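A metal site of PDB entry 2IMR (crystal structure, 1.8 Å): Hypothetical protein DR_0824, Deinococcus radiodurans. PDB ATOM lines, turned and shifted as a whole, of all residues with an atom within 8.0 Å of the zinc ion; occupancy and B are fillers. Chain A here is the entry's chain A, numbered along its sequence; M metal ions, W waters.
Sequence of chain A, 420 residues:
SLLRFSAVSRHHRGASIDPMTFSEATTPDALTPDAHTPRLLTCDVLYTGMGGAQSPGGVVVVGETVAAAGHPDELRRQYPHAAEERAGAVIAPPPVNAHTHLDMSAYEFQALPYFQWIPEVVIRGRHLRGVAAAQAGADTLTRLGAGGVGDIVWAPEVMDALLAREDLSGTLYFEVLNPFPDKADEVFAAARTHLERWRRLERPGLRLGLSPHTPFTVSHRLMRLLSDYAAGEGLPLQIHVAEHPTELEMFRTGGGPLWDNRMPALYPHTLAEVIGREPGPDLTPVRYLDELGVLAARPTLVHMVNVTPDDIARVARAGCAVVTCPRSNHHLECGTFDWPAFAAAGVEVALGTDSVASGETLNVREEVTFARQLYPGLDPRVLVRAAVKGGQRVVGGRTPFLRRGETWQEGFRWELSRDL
Water W1 bridges OD1 of Asp 354 (2.5 Å) and NE2 of His 303 (3.0 Å).
Water W1 is bound to the zinc ion.
NE2 of His 101 is bound to the zinc ion.
NE2 of His 240 is bound to the zinc ion (2.1 Å).
The zinc ion is bound by NE2 of His 99.
OD1 of Asp 354 touches the zinc ion, 3.3 Å away.
Within 4 Å of the zinc ion: His 99, His 101, His 240 and Asp 354.
The nearest printed residue that does not touch the zinc ion is His 303 (4.4 Å).
The side-chain carboxylate (OD2) of Asp 354 lies within hydrogen-bond range of the side-chain hydroxyl (OG) of Ser 328, 2.7 Å away.
N of Thr 353 is in hydrogen-bond range of O of His 99.
A ring nitrogen (ND1) of His 99 sits at hydrogen-bond distance from the side-chain amide oxygen (OE1) of Gln 238, 2.6 Å away.
N of Asp 354 is in hydrogen-bond range of O of His 99 (2.8 Å).
A ring nitrogen (ND1) of His 240 sits at hydrogen-bond distance from the backbone carbonyl oxygen (O) of His 213 (2.8 Å).
O of Asp 354 is in hydrogen-bond range of OG1 of Thr 100 (3.0 Å).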
ATOM      1  N   HIS A  99       4.759  20.795  -7.513  1.00  0.00           N
ATOM      2  CA  HIS A  99       3.526  20.963  -6.775  1.00  0.00           C
ATOM      3  C   HIS A  99       3.538  22.160  -5.841  1.00  0.00           C
ATOM      4  O   HIS A  99       4.347  22.230  -4.918  1.00  0.00           O
ATOM      5  CB  HIS A  99       3.180  19.721  -5.940  1.00  0.00           C
ATOM      6  CG  HIS A  99       1.853  19.811  -5.249  1.00  0.00           C
ATOM      7  ND1 HIS A  99       0.661  19.506  -5.879  1.00  0.00           N
ATOM      8  CD2 HIS A  99       1.519  20.254  -4.012  1.00  0.00           C
ATOM      9  CE1 HIS A  99      -0.349  19.752  -5.070  1.00  0.00           C
ATOM     10  NE2 HIS A  99       0.146  20.204  -3.925  1.00  0.00           N
ATOM     11  N   THR A 100       2.634  23.096  -6.101  1.00  0.00           N
ATOM     12  CA  THR A 100       2.479  24.259  -5.251  1.00  0.00           C
ATOM     13  C   THR A 100       1.084  24.837  -5.476  1.00  0.00           C
ATOM     14  O   THR A 100       0.340  24.359  -6.343  1.00  0.00           O
ATOM     15  CB  THR A 100       3.540  25.353  -5.562  1.00  0.00           C
ATOM     16  OG1 THR A 100       3.415  26.416  -4.603  1.00  0.00           O
ATOM     17  CG2 THR A 100       3.353  25.920  -6.956  1.00  0.00           C
ATOM     18  N   HIS A 101       0.727  25.818  -4.664  1.00  0.00           N
ATOM     19  CA  HIS A 101      -0.555  26.501  -4.793  1.00  0.00           C
ATOM     20  C   HIS A 101      -0.191  27.979  -4.774  1.00  0.00           C
ATOM     21  O   HIS A 101       0.271  28.476  -3.743  1.00  0.00           O
ATOM     22  CB  HIS A 101      -1.485  26.211  -3.602  1.00  0.00           C
ATOM     23  CG  HIS A 101      -1.946  24.793  -3.498  1.00  0.00           C
ATOM     24  ND1 HIS A 101      -3.279  24.439  -3.590  1.00  0.00           N
ATOM     25  CD2 HIS A 101      -1.278  23.647  -3.221  1.00  0.00           C
ATOM     26  CE1 HIS A 101      -3.406  23.145  -3.375  1.00  0.00           C
ATOM     27  NE2 HIS A 101      -2.206  22.639  -3.153  1.00  0.00           N
ATOM     28  N   MET A 104      -5.028  30.035  -2.990  1.00  0.00           N
ATOM     29  CA  MET A 104      -5.777  29.030  -2.234  1.00  0.00           C
ATOM     30  C   MET A 104      -7.084  29.616  -1.716  1.00  0.00           C
ATOM     31  O   MET A 104      -7.385  30.787  -1.942  1.00  0.00           O
ATOM     32  CB  MET A 104      -4.952  28.496  -1.059  1.00  0.00           C
ATOM     33  CG  MET A 104      -3.656  27.800  -1.452  1.00  0.00           C
ATOM     34  SD  MET A 104      -2.722  27.140  -0.040  1.00  0.00           S
ATOM     35  CE  MET A 104      -3.672  25.660   0.341  1.00  0.00           C
ATOM     36  N   GLU A 108     -10.438  25.295   1.487  1.00  0.00           N
ATOM     37  CA  GLU A 108      -9.591  24.104   1.556  1.00  0.00           C
ATOM     38  C   GLU A 108      -8.833  24.008   2.877  1.00  0.00           C
ATOM     39  O   GLU A 108      -8.424  22.912   3.271  1.00  0.00           O
ATOM     40  CB  GLU A 108      -8.661  24.026   0.334  1.00  0.00           C
ATOM     41  CG  GLU A 108      -7.683  25.156   0.134  1.00  0.00           C
ATOM     42  CD  GLU A 108      -7.086  25.155  -1.267  1.00  0.00           C
ATOM     43  OE1 GLU A 108      -6.575  24.100  -1.723  1.00  0.00           O
ATOM     44  OE2 GLU A 108      -7.116  26.212  -1.918  1.00  0.00           O
ATOM     45  N   LEU A 112      -9.540  20.768   5.982  1.00  0.00           N
ATOM     46  CA  LEU A 112      -8.475  19.925   6.520  1.00  0.00           C
ATOM     47  C   LEU A 112      -8.070  20.290   7.959  1.00  0.00           C
ATOM     48  O   LEU A 112      -7.295  21.223   8.181  1.00  0.00           O
ATOM     49  CB  LEU A 112      -7.263  20.001   5.591  1.00  0.00           C
ATOM     50  CG  LEU A 112      -7.574  19.728   4.110  1.00  0.00           C
ATOM     51  CD1 LEU A 112      -6.284  19.721   3.294  1.00  0.00           C
ATOM     52  CD2 LEU A 112      -8.289  18.387   3.976  1.00  0.00           C
ATOM     53  N   PHE A 115      -4.453  21.176   9.230  1.00  0.00           N
ATOM     54  CA  PHE A 115      -3.866  22.444   8.833  1.00  0.00           C
ATOM     55  C   PHE A 115      -4.106  23.425   9.974  1.00  0.00           C
ATOM     56  O   PHE A 115      -3.268  24.267  10.287  1.00  0.00           O
ATOM     57  CB  PHE A 115      -4.517  22.997   7.557  1.00  0.00           C
ATOM     58  CG  PHE A 115      -3.774  22.645   6.295  1.00  0.00           C
ATOM     59  CD1 PHE A 115      -3.656  21.327   5.875  1.00  0.00           C
ATOM     60  CD2 PHE A 115      -3.195  23.646   5.520  1.00  0.00           C
ATOM     61  CE1 PHE A 115      -2.982  21.006   4.708  1.00  0.00           C
ATOM     62  CE2 PHE A 115      -2.503  23.338   4.352  1.00  0.00           C
ATOM     63  CZ  PHE A 115      -2.405  22.011   3.941  1.00  0.00           C
ATOM     64  N   GLY A 150       4.048  22.919 -11.372  1.00  0.00           N
ATOM     65  CA  GLY A 150       2.821  22.147 -11.322  1.00  0.00           C
ATOM     66  C   GLY A 150       2.008  22.913 -10.299  1.00  0.00           C
ATOM     67  O   GLY A 150       2.163  22.725  -9.095  1.00  0.00           O
ATOM     68  N   ASP A 151       1.141  23.808 -10.773  1.00  0.00           N
ATOM     69  CA  ASP A 151       0.356  24.641  -9.881  1.00  0.00           C
ATOM     70  C   ASP A 151      -1.106  24.260  -9.745  1.00  0.00           C
ATOM     71  O   ASP A 151      -1.801  24.043 -10.742  1.00  0.00           O
ATOM     72  CB  ASP A 151       0.449  26.105 -10.320  1.00  0.00           C
ATOM     73  CG  ASP A 151      -0.325  27.042  -9.403  1.00  0.00           C
ATOM     74  OD1 ASP A 151      -0.096  26.961  -8.184  1.00  0.00           O
ATOM     75  OD2 ASP A 151      -1.137  27.856  -9.885  1.00  0.00           O
ATOM     76  N   ILE A 152      -1.565  24.184  -8.507  1.00  0.00           N
ATOM     77  CA  ILE A 152      -2.947  23.870  -8.218  1.00  0.00           C
ATOM     78  C   ILE A 152      -3.655  25.217  -8.137  1.00  0.00           C
ATOM     79  O   ILE A 152      -3.253  26.088  -7.374  1.00  0.00           O
ATOM     80  CB  ILE A 152      -3.104  23.131  -6.879  1.00  0.00           C
ATOM     81  CG1 ILE A 152      -2.228  21.872  -6.869  1.00  0.00           C
ATOM     82  CG2 ILE A 152      -4.573  22.769  -6.645  1.00  0.00           C
ATOM     83  CD1 ILE A 152      -2.459  20.940  -8.059  1.00  0.00           C
ATOM     84  N   GLU A 175      -8.460  22.950  -9.269  1.00  0.00           N
ATOM     85  CA  GLU A 175      -8.864  22.135  -8.124  1.00  0.00           C
ATOM     86  C   GLU A 175     -10.378  22.007  -7.966  1.00  0.00           C
ATOM     87  O   GLU A 175     -11.105  22.988  -8.079  1.00  0.00           O
ATOM     88  CB  GLU A 175      -8.253  22.705  -6.843  1.00  0.00           C
ATOM     89  CG  GLU A 175      -8.220  21.705  -5.701  1.00  0.00           C
ATOM     90  CD  GLU A 175      -7.414  22.215  -4.515  1.00  0.00           C
ATOM     91  OE1 GLU A 175      -7.816  23.229  -3.921  1.00  0.00           O
ATOM     92  OE2 GLU A 175      -6.374  21.606  -4.198  1.00  0.00           O
ATOM     93  N   SER A 211      -7.426  18.745 -10.797  1.00  0.00           N
ATOM     94  CA  SER A 211      -6.996  18.272  -9.490  1.00  0.00           C
ATOM     95  C   SER A 211      -8.094  17.979  -8.488  1.00  0.00           C
ATOM     96  O   SER A 211      -8.573  18.883  -7.813  1.00  0.00           O
ATOM     97  CB  SER A 211      -6.020  19.257  -8.866  1.00  0.00           C
ATOM     98  OG  SER A 211      -5.680  18.837  -7.559  1.00  0.00           O
ATOM     99  N   HIS A 213      -9.299  17.376  -5.226  1.00  0.00           N
ATOM    100  CA  HIS A 213      -8.621  17.726  -3.964  1.00  0.00           C
ATOM    101  C   HIS A 213      -7.971  16.574  -3.192  1.00  0.00           C
ATOM    102  O   HIS A 213      -6.748  16.497  -3.091  1.00  0.00           O
ATOM    103  CB  HIS A 213      -9.593  18.501  -3.058  1.00  0.00           C
ATOM    104  CG  HIS A 213      -8.939  19.141  -1.874  1.00  0.00           C
ATOM    105  ND1 HIS A 213      -9.486  19.076  -0.603  1.00  0.00           N
ATOM    106  CD2 HIS A 213      -7.823  19.895  -1.770  1.00  0.00           C
ATOM    107  CE1 HIS A 213      -8.728  19.764   0.226  1.00  0.00           C
ATOM    108  NE2 HIS A 213      -7.709  20.275  -0.452  1.00  0.00           N
ATOM    109  N   GLN A 238      -3.652  15.478 -10.682  1.00  0.00           N
ATOM    110  CA  GLN A 238      -2.882  15.523  -9.452  1.00  0.00           C
ATOM    111  C   GLN A 238      -3.902  15.413  -8.330  1.00  0.00           C
ATOM    112  O   GLN A 238      -4.905  16.139  -8.314  1.00  0.00           O
ATOM    113  CB  GLN A 238      -2.059  16.808  -9.302  1.00  0.00           C
ATOM    114  CG  GLN A 238      -0.588  16.605  -9.658  1.00  0.00           C
ATOM    115  CD  GLN A 238       0.314  17.755  -9.190  1.00  0.00           C
ATOM    116  OE1 GLN A 238       0.172  18.262  -8.084  1.00  0.00           O
ATOM    117  NE2 GLN A 238       1.263  18.134 -10.034  1.00  0.00           N
ATOM    118  N   ILE A 239      -3.681  14.466  -7.421  1.00  0.00           N
ATOM    119  CA  ILE A 239      -4.560  14.227  -6.288  1.00  0.00           C
ATOM    120  C   ILE A 239      -3.700  14.180  -5.015  1.00  0.00           C
ATOM    121  O   ILE A 239      -2.671  13.518  -5.002  1.00  0.00           O
ATOM    122  CB  ILE A 239      -5.293  12.857  -6.407  1.00  0.00           C
ATOM    123  CG1 ILE A 239      -5.982  12.737  -7.769  1.00  0.00           C
ATOM    124  CG2 ILE A 239      -6.316  12.695  -5.280  1.00  0.00           C
ATOM    125  CD1 ILE A 239      -6.547  11.348  -8.042  1.00  0.00           C
ATOM    126  N   HIS A 240      -4.092  14.912  -3.978  1.00  0.00           N
ATOM    127  CA  HIS A 240      -3.355  14.871  -2.708  1.00  0.00           C
ATOM    128  C   HIS A 240      -3.797  13.592  -2.027  1.00  0.00           C
ATOM    129  O   HIS A 240      -4.989  13.420  -1.786  1.00  0.00           O
ATOM    130  CB  HIS A 240      -3.725  16.041  -1.794  1.00  0.00           C
ATOM    131  CG  HIS A 240      -3.483  17.393  -2.375  1.00  0.00           C
ATOM    132  ND1 HIS A 240      -4.448  18.079  -3.081  1.00  0.00           N
ATOM    133  CD2 HIS A 240      -2.398  18.201  -2.324  1.00  0.00           C
ATOM    134  CE1 HIS A 240      -3.976  19.260  -3.442  1.00  0.00           C
ATOM    135  NE2 HIS A 240      -2.736  19.356  -2.996  1.00  0.00           N
ATOM    136  N   GLU A 243      -1.721  12.382   2.971  1.00  0.00           N
ATOM    137  CA  GLU A 243      -0.805  13.399   3.481  1.00  0.00           C
ATOM    138  C   GLU A 243      -0.540  13.293   4.978  1.00  0.00           C
ATOM    139  O   GLU A 243       0.614  13.244   5.397  1.00  0.00           O
ATOM    140  CB  GLU A 243      -1.332  14.808   3.154  1.00  0.00           C
ATOM    141  CG  GLU A 243      -0.423  15.916   3.688  1.00  0.00           C
ATOM    142  CD  GLU A 243      -0.900  17.305   3.313  1.00  0.00           C
ATOM    143  OE1 GLU A 243      -2.106  17.449   3.015  1.00  0.00           O
ATOM    144  OE2 GLU A 243      -0.076  18.244   3.330  1.00  0.00           O
ATOM    145  N   VAL A 302       0.095  13.217  -4.877  1.00  0.00           N
ATOM    146  CA  VAL A 302       0.890  14.138  -4.056  1.00  0.00           C
ATOM    147  C   VAL A 302       0.948  13.795  -2.571  1.00  0.00           C
ATOM    148  O   VAL A 302      -0.052  13.375  -1.978  1.00  0.00           O
ATOM    149  CB  VAL A 302       0.348  15.571  -4.234  1.00  0.00           C
ATOM    150  CG1 VAL A 302       1.258  16.560  -3.506  1.00  0.00           C
ATOM    151  CG2 VAL A 302       0.262  15.900  -5.721  1.00  0.00           C
ATOM    152  N   HIS A 303       2.134  13.989  -1.994  1.00  0.00           N
ATOM    153  CA  HIS A 303       2.425  13.722  -0.583  1.00  0.00           C
ATOM    154  C   HIS A 303       2.672  12.239  -0.360  1.00  0.00           C
ATOM    155  O   HIS A 303       3.820  11.827  -0.229  1.00  0.00           O
ATOM    156  CB  HIS A 303       1.307  14.266   0.310  1.00  0.00           C
ATOM    157  CG  HIS A 303       1.176  15.764   0.263  1.00  0.00           C
ATOM    158  ND1 HIS A 303       2.254  16.601   0.474  1.00  0.00           N
ATOM    159  CD2 HIS A 303       0.121  16.556  -0.003  1.00  0.00           C
ATOM    160  CE1 HIS A 303       1.856  17.860   0.331  1.00  0.00           C
ATOM    161  NE2 HIS A 303       0.569  17.860   0.039  1.00  0.00           N
ATOM    162  N   CYS A 325       6.743  16.808  -1.017  1.00  0.00           N
ATOM    163  CA  CYS A 325       7.014  18.180  -0.593  1.00  0.00           C
ATOM    164  C   CYS A 325       7.617  18.075   0.819  1.00  0.00           C
ATOM    165  O   CYS A 325       6.908  18.181   1.820  1.00  0.00           O
ATOM    166  CB  CYS A 325       5.708  18.997  -0.554  1.00  0.00           C
ATOM    167  SG  CYS A 325       4.770  19.028  -2.122  1.00  0.00           S
ATOM    168  N   SER A 328       7.109  21.008   3.628  1.00  0.00           N
ATOM    169  CA  SER A 328       5.693  21.072   3.961  1.00  0.00           C
ATOM    170  C   SER A 328       5.290  19.925   4.885  1.00  0.00           C
ATOM    171  O   SER A 328       4.605  20.148   5.878  1.00  0.00           O
ATOM    172  CB  SER A 328       4.849  21.025   2.686  1.00  0.00           C
ATOM    173  OG  SER A 328       3.467  21.079   3.006  1.00  0.00           O
ATOM    174  N   THR A 353       7.283  22.186  -3.451  1.00  0.00           N
ATOM    175  CA  THR A 353       7.474  22.922  -2.201  1.00  0.00           C
ATOM    176  C   THR A 353       6.127  23.073  -1.511  1.00  0.00           C
ATOM    177  O   THR A 353       6.061  23.421  -0.334  1.00  0.00           O
ATOM    178  CB  THR A 353       8.005  24.354  -2.455  1.00  0.00           C
ATOM    179  OG1 THR A 353       7.048  25.065  -3.252  1.00  0.00           O
ATOM    180  CG2 THR A 353       9.340  24.314  -3.190  1.00  0.00           C
ATOM    181  N   ASP A 354       5.057  22.818  -2.260  1.00  0.00           N
ATOM    182  CA  ASP A 354       3.693  22.992  -1.760  1.00  0.00           C
ATOM    183  C   ASP A 354       3.567  24.523  -1.667  1.00  0.00           C
ATOM    184  O   ASP A 354       4.504  25.224  -2.046  1.00  0.00           O
ATOM    185  CB  ASP A 354       3.515  22.349  -0.379  1.00  0.00           C
ATOM    186  CG  ASP A 354       2.102  21.880  -0.135  1.00  0.00           C
ATOM    187  OD1 ASP A 354       1.203  22.257  -0.908  1.00  0.00           O
ATOM    188  OD2 ASP A 354       1.892  21.150   0.842  1.00  0.00           O
ATOM    189  N   SER A 355       2.451  25.051  -1.202  1.00  0.00           N
ATOM    190  CA  SER A 355       2.304  26.501  -1.090  1.00  0.00           C
ATOM    191  C   SER A 355       3.293  27.003  -0.026  1.00  0.00           C
ATOM    192  O   SER A 355       3.776  26.227   0.796  1.00  0.00           O
ATOM    193  CB  SER A 355       0.879  26.886  -0.673  1.00  0.00           C
ATOM    194  OG  SER A 355       0.745  26.866   0.736  1.00  0.00           O
ATOM    195  N   SER A 358       3.052  26.359   4.051  1.00  0.00           N
ATOM    196  CA  SER A 358       3.675  25.245   4.754  1.00  0.00           C
ATOM    197  C   SER A 358       5.054  24.872   4.219  1.00  0.00           C
ATOM    198  O   SER A 358       5.829  24.189   4.900  1.00  0.00           O
ATOM    199  CB  SER A 358       2.768  24.007   4.713  1.00  0.00           C
ATOM    200  OG  SER A 358       2.589  23.531   3.379  1.00  0.00           O
HETATM  201 ZN    ZN M   1      -1.353  20.856  -2.552  1.00  0.00          ZN
HETATM  202  O   HOH W   1      -0.551  20.458  -0.997  1.00  0.00           O
HETATM  203  O   HOH W   2      -3.352  21.301   0.058  1.00  0.00           O
